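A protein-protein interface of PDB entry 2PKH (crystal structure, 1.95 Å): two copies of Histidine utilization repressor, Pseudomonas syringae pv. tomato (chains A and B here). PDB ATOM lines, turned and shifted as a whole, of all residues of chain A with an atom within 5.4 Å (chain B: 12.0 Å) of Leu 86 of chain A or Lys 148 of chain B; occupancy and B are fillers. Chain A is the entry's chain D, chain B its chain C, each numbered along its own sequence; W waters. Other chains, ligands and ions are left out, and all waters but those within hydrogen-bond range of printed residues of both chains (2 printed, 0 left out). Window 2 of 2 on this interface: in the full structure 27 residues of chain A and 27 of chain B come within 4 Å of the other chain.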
ATOM      1  N   TYR A  77      23.013  24.216 -14.435  1.00  0.00           N
ATOM      2  CA  TYR A  77      23.215  22.969 -13.709  1.00  0.00           C
ATOM      3  C   TYR A  77      22.483  23.034 -12.329  1.00  0.00           C
ATOM      4  O   TYR A  77      21.812  22.080 -11.887  1.00  0.00           O
ATOM      5  CB  TYR A  77      24.766  22.626 -13.571  1.00  0.00           C
ATOM      6  CG  TYR A  77      24.956  21.304 -12.839  1.00  0.00           C
ATOM      7  CD1 TYR A  77      24.887  20.116 -13.531  1.00  0.00           C
ATOM      8  CD2 TYR A  77      25.058  21.261 -11.441  1.00  0.00           C
ATOM      9  CE1 TYR A  77      24.952  18.925 -12.884  1.00  0.00           C
ATOM     10  CE2 TYR A  77      25.102  20.041 -10.754  1.00  0.00           C
ATOM     11  CZ  TYR A  77      25.051  18.888 -11.499  1.00  0.00           C
ATOM     12  OH  TYR A  77      25.104  17.697 -10.882  1.00  0.00           O
ATOM     13  N   LEU A  80      18.904  22.688 -12.876  1.00  0.00           N
ATOM     14  CA  LEU A  80      18.440  21.288 -13.077  1.00  0.00           C
ATOM     15  C   LEU A  80      18.488  20.437 -11.789  1.00  0.00           C
ATOM     16  O   LEU A  80      17.657  19.526 -11.595  1.00  0.00           O
ATOM     17  CB  LEU A  80      19.137  20.576 -14.214  1.00  0.00           C
ATOM     18  CG  LEU A  80      19.011  21.255 -15.580  1.00  0.00           C
ATOM     19  CD1 LEU A  80      20.158  20.749 -16.487  1.00  0.00           C
ATOM     20  CD2 LEU A  80      17.556  20.985 -16.082  1.00  0.00           C
ATOM     21  N   SER A  81      19.438  20.767 -10.924  1.00  0.00           N
ATOM     22  CA  SER A  81      19.613  20.083  -9.643  1.00  0.00           C
ATOM     23  C   SER A  81      18.369  20.127  -8.845  1.00  0.00           C
ATOM     24  O   SER A  81      18.141  19.258  -7.992  1.00  0.00           O
ATOM     25  CB  SER A  81      20.654  20.808  -8.780  1.00  0.00           C
ATOM     26  OG  SER A  81      21.932  20.384  -9.172  1.00  0.00           O
ATOM     27  N   ALA A  84      15.098  17.778 -10.718  1.00  0.00           N
ATOM     28  CA  ALA A  84      15.168  16.318 -10.696  1.00  0.00           C
ATOM     29  C   ALA A  84      16.391  15.958  -9.892  1.00  0.00           C
ATOM     30  O   ALA A  84      17.368  16.702  -9.894  1.00  0.00           O
ATOM     31  CB  ALA A  84      15.282  15.718 -12.121  1.00  0.00           C
ATOM     32  N   PRO A  85      16.320  14.823  -9.169  1.00  0.00           N
ATOM     33  CA  PRO A  85      17.512  14.407  -8.420  1.00  0.00           C
ATOM     34  C   PRO A  85      18.561  13.974  -9.423  1.00  0.00           C
ATOM     35  O   PRO A  85      18.308  13.060 -10.199  1.00  0.00           O
ATOM     36  CB  PRO A  85      17.030  13.212  -7.606  1.00  0.00           C
ATOM     37  CG  PRO A  85      15.740  12.735  -8.263  1.00  0.00           C
ATOM     38  CD  PRO A  85      15.175  13.894  -9.040  1.00  0.00           C
ATOM     39  N   LEU A  86      19.672  14.679  -9.447  1.00  0.00           N
ATOM     40  CA  LEU A  86      20.821  14.358 -10.323  1.00  0.00           C
ATOM     41  C   LEU A  86      21.753  13.476  -9.538  1.00  0.00           C
ATOM     42  O   LEU A  86      22.237  13.898  -8.487  1.00  0.00           O
ATOM     43  CB  LEU A  86      21.515  15.638 -10.793  1.00  0.00           C
ATOM     44  CG  LEU A  86      20.620  16.706 -11.489  1.00  0.00           C
ATOM     45  CD1 LEU A  86      21.579  17.821 -11.884  1.00  0.00           C
ATOM     46  CD2 LEU A  86      19.859  16.157 -12.717  1.00  0.00           C
ATOM     47  N   THR A  87      21.935  12.237 -10.005  1.00  0.00           N
ATOM     48  CA  THR A  87      22.567  11.170  -9.175  1.00  0.00           C
ATOM     49  C   THR A  87      23.921  10.633  -9.650  1.00  0.00           C
ATOM     50  O   THR A  87      24.661  10.017  -8.877  1.00  0.00           O
ATOM     51  CB  THR A  87      21.614   9.989  -9.048  1.00  0.00           C
ATOM     52  OG1 THR A  87      21.199   9.584 -10.372  1.00  0.00           O
ATOM     53  CG2 THR A  87      20.368  10.378  -8.174  1.00  0.00           C
ATOM     54  N   GLU A  88      24.230  10.860 -10.935  1.00  0.00           N
ATOM     55  CA  GLU A  88      25.450  10.332 -11.590  1.00  0.00           C
ATOM     56  C   GLU A  88      25.828  11.242 -12.737  1.00  0.00           C
ATOM     57  O   GLU A  88      24.933  11.799 -13.406  1.00  0.00           O
ATOM     58  CB  GLU A  88      25.153   8.958 -12.124  1.00  0.00           C
ATOM     59  CG  GLU A  88      26.353   8.203 -12.603  1.00  0.00           C
ATOM     60  CD  GLU A  88      26.227   6.747 -12.251  1.00  0.00           C
ATOM     61  OE1 GLU A  88      25.086   6.330 -11.947  1.00  0.00           O
ATOM     62  OE2 GLU A  88      27.265   6.037 -12.251  1.00  0.00           O
ATOM     63  N   GLY A  89      27.131  11.441 -12.939  1.00  0.00           N
ATOM     64  CA  GLY A  89      27.634  12.241 -14.063  1.00  0.00           C
ATOM     65  C   GLY A  89      28.804  11.531 -14.762  1.00  0.00           C
ATOM     66  O   GLY A  89      29.528  10.781 -14.142  1.00  0.00           O
ATOM     67  N   THR A 121      24.758  14.098 -17.435  1.00  0.00           N
ATOM     68  CA  THR A 121      24.256  13.870 -16.093  1.00  0.00           C
ATOM     69  C   THR A 121      22.914  13.115 -16.140  1.00  0.00           C
ATOM     70  O   THR A 121      22.070  13.330 -17.040  1.00  0.00           O
ATOM     71  CB  THR A 121      24.025  15.224 -15.339  1.00  0.00           C
ATOM     72  OG1 THR A 121      25.236  15.982 -15.334  1.00  0.00           O
ATOM     73  CG2 THR A 121      23.629  14.982 -13.961  1.00  0.00           C
ATOM     74  N   TRP A 122      22.746  12.262 -15.129  1.00  0.00           N
ATOM     75  CA  TRP A 122      21.682  11.297 -15.050  1.00  0.00           C
ATOM     76  C   TRP A 122      20.873  11.449 -13.789  1.00  0.00           C
ATOM     77  O   TRP A 122      21.416  11.834 -12.734  1.00  0.00           O
ATOM     78  CB  TRP A 122      22.267   9.906 -15.009  1.00  0.00           C
ATOM     79  CG  TRP A 122      23.099   9.492 -16.201  1.00  0.00           C
ATOM     80  CD1 TRP A 122      24.366   9.886 -16.523  1.00  0.00           C
ATOM     81  CD2 TRP A 122      22.714   8.512 -17.163  1.00  0.00           C
ATOM     82  NE1 TRP A 122      24.788   9.219 -17.668  1.00  0.00           N
ATOM     83  CE2 TRP A 122      23.779   8.368 -18.066  1.00  0.00           C
ATOM     84  CE3 TRP A 122      21.557   7.734 -17.338  1.00  0.00           C
ATOM     85  CZ2 TRP A 122      23.718   7.481 -19.155  1.00  0.00           C
ATOM     86  CZ3 TRP A 122      21.498   6.836 -18.427  1.00  0.00           C
ATOM     87  CH2 TRP A 122      22.573   6.723 -19.312  1.00  0.00           C
ATOM     88  N   SER A 123      19.575  11.120 -13.926  1.00  0.00           N
ATOM     89  CA  SER A 123      18.644  10.990 -12.782  1.00  0.00           C
ATOM     90  C   SER A 123      18.267   9.551 -12.731  1.00  0.00           C
ATOM     91  O   SER A 123      17.424   9.095 -13.512  1.00  0.00           O
ATOM     92  CB  SER A 123      17.379  11.824 -12.969  1.00  0.00           C
ATOM     93  OG  SER A 123      16.772  11.982 -11.700  1.00  0.00           O
ATOM     94  N   VAL A 128      19.573  13.016 -18.469  1.00  0.00           N
ATOM     95  CA  VAL A 128      18.815  14.175 -18.338  1.00  0.00           C
ATOM     96  C   VAL A 128      19.403  15.326 -19.209  1.00  0.00           C
ATOM     97  O   VAL A 128      18.634  16.024 -19.951  1.00  0.00           O
ATOM     98  CB  VAL A 128      18.765  14.540 -16.879  1.00  0.00           C
ATOM     99  CG1 VAL A 128      18.500  16.022 -16.656  1.00  0.00           C
ATOM    100  CG2 VAL A 128      17.659  13.728 -16.251  1.00  0.00           C
ATOM    101  N   GLY B 144      35.665   9.649 -17.169  1.00  0.00           N
ATOM    102  CA  GLY B 144      35.223   8.995 -15.931  1.00  0.00           C
ATOM    103  C   GLY B 144      33.776   9.151 -15.622  1.00  0.00           C
ATOM    104  O   GLY B 144      33.067   9.908 -16.302  1.00  0.00           O
ATOM    105  N   ARG B 145      33.335   8.462 -14.574  1.00  0.00           N
ATOM    106  CA  ARG B 145      31.936   8.541 -14.153  1.00  0.00           C
ATOM    107  C   ARG B 145      31.929   8.531 -12.627  1.00  0.00           C
ATOM    108  O   ARG B 145      32.734   7.826 -12.022  1.00  0.00           O
ATOM    109  CB  ARG B 145      31.194   7.349 -14.746  1.00  0.00           C
ATOM    110  CG  ARG B 145      29.844   7.055 -14.188  1.00  0.00           C
ATOM    111  CD  ARG B 145      29.264   5.812 -14.840  1.00  0.00           C
ATOM    112  NE  ARG B 145      29.785   4.576 -14.245  1.00  0.00           N
ATOM    113  CZ  ARG B 145      30.511   3.669 -14.902  1.00  0.00           C
ATOM    114  NH1 ARG B 145      30.800   3.825 -16.201  1.00  0.00           N
ATOM    115  NH2 ARG B 145      30.923   2.596 -14.262  1.00  0.00           N
ATOM    116  N   PHE B 146      31.034   9.310 -12.019  1.00  0.00           N
ATOM    117  CA  PHE B 146      31.023   9.531 -10.571  1.00  0.00           C
ATOM    118  C   PHE B 146      29.615   9.717 -10.048  1.00  0.00           C
ATOM    119  O   PHE B 146      28.789  10.406 -10.685  1.00  0.00           O
ATOM    120  CB  PHE B 146      31.763  10.818 -10.281  1.00  0.00           C
ATOM    121  CG  PHE B 146      31.341  11.985 -11.189  1.00  0.00           C
ATOM    122  CD1 PHE B 146      30.293  12.864 -10.810  1.00  0.00           C
ATOM    123  CD2 PHE B 146      32.011  12.232 -12.410  1.00  0.00           C
ATOM    124  CE1 PHE B 146      29.903  13.949 -11.620  1.00  0.00           C
ATOM    125  CE2 PHE B 146      31.612  13.318 -13.250  1.00  0.00           C
ATOM    126  CZ  PHE B 146      30.566  14.173 -12.823  1.00  0.00           C
ATOM    127  N   THR B 147      29.290   9.138  -8.913  1.00  0.00           N
ATOM    128  CA  THR B 147      27.983   9.468  -8.317  1.00  0.00           C
ATOM    129  C   THR B 147      28.040  10.867  -7.655  1.00  0.00           C
ATOM    130  O   THR B 147      29.145  11.450  -7.498  1.00  0.00           O
ATOM    131  CB  THR B 147      27.498   8.430  -7.329  1.00  0.00           C
ATOM    132  OG1 THR B 147      28.587   8.103  -6.472  1.00  0.00           O
ATOM    133  CG2 THR B 147      27.028   7.163  -8.042  1.00  0.00           C
ATOM    134  N   LYS B 148      26.856  11.381  -7.291  1.00  0.00           N
ATOM    135  CA  LYS B 148      26.665  12.771  -6.890  1.00  0.00           C
ATOM    136  C   LYS B 148      25.954  12.878  -5.557  1.00  0.00           C
ATOM    137  O   LYS B 148      26.103  11.996  -4.717  1.00  0.00           O
ATOM    138  CB  LYS B 148      25.755  13.472  -7.880  1.00  0.00           C
ATOM    139  CG  LYS B 148      26.466  14.220  -8.932  1.00  0.00           C
ATOM    140  CD  LYS B 148      25.551  14.463 -10.077  1.00  0.00           C
ATOM    141  CE  LYS B 148      26.400  14.633 -11.320  1.00  0.00           C
ATOM    142  NZ  LYS B 148      27.087  15.962 -11.338  1.00  0.00           N
HETATM  143  O   HOH W   1      27.632  16.208 -14.040  1.00  0.00           O
HETATM  144  O   HOH W   2      24.115   9.623  -5.975  1.00  0.00           O
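Leu 86 of chain A touches one residue of chain B. Lys 148 of chain B touches just these residues of chain A: Tyr 77, Leu 86, Thr 87, Glu 88, Gly 89 and Thr 121. No residue of chain B comes within 4 Å of Leu 80 of chain A. Thr 87 of chain A touches just these residues of chain B: Thr 147 (3.4 Å) and Lys 148 (3.0 Å). Of chain B, only Arg 145, Phe 146 and Lys 148 come within 4 Å of Glu 88 of chain A. No residue of chain B comes within 4 Å of Ser 123 of chain A. No residue of chain B comes within 4 Å of Val 128 of chain A. Of the printed residues of chain A, Phe 146 of chain B touches Glu 88 (3.5 Å) and Gly 89 (3.0 Å). Of the printed residues of chain A, Arg 145 of chain B touches Glu 88 (3.3 Å) and Gly 89 (3.3 Å). Gly 144 of chain B touches none of the printed residues of chain A. The nearest residue of chain B that does not touch Leu 86 of chain A is Thr 147 of chain B (6.6 Å). The nearest printed residue of chain A that does not touch Lys 148 of chain B is Trp 122 of chain A (5.6 Å). The nearest printed residue of chain A that does not touch Phe 146 of chain B is Thr 87 of chain A (4.5 Å).
Lys 148 of chain B touches Leu 86 of chain A (CB to O, 3.6 Å). Thr 147 of chain B touches Thr 87 of chain A (CA to O, 3.4 Å). Glu 88 of chain A touches Phe 146 of chain B (CA to O, 3.5 Å). Glu 88 of chain A touches Lys 148 of chain B (C to CE, 3.7 Å). Arg 145 of chain B touches Gly 89 of chain A (CA to O, 3.3 Å). Gly 89 of chain A touches Lys 148 of chain B. Lys 148 of chain B touches Thr 121 of chain A (CE to CG2, 3.8 Å).
No position is printed for both chains. Of the 11 pairs that touch across the chains among the printed residues, none has its exchanged pair printed and touching as well.
The guanidinium group of Arg 145 of chain B is in salt-bridge range of the side-chain carboxylate of Glu 88 of chain A (3.5 Å). The backbone carbonyl oxygen of Phe 146 of chain B lies within hydrogen-bond range of the backbone NH of Gly 89 of chain A, 3.0 Å away. NZ of Lys 148 of chain B is in hydrogen-bond range of OH of Tyr 77 of chain A. N of Lys 148 of chain B is in hydrogen-bond range of O of Thr 87 of chain A, 3.0 Å away.
Water W1 lies within hydrogen-bond range of OG1 of Thr 121 of chain A and NZ of Lys 148 of chain B. Water W2 bridges O of Thr 87 of chain A and O of Lys 148 of chain B.
Of the 13 printed residues of chain A, 6 touch a printed residue of chain B. Hydrophobic or aromatic side chains of chain A within 4 Å of the printed part of chain B: Tyr 77. Hydrophobic or aromatic side chains of chain B within 4 Å of the printed part of chain A: Phe 146.
OG of Ser 81 of chain A is in hydrogen-bond range of O of Tyr 77 of chain A (3.2 Å). The backbone carbonyl oxygen (O) of Trp 122 of chain A lies within hydrogen-bond range of the backbone NH (N) of Thr 87 of chain A, 2.8 Å away. N of Trp 122 of chain A sits at hydrogen-bond distance from O of Glu 88 of chain A (2.8 Å). The backbone carbonyl oxygen of Thr 121 of chain A sits at hydrogen-bond distance from the backbone NH of Val 128 of chain A, at 2.9 Å.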
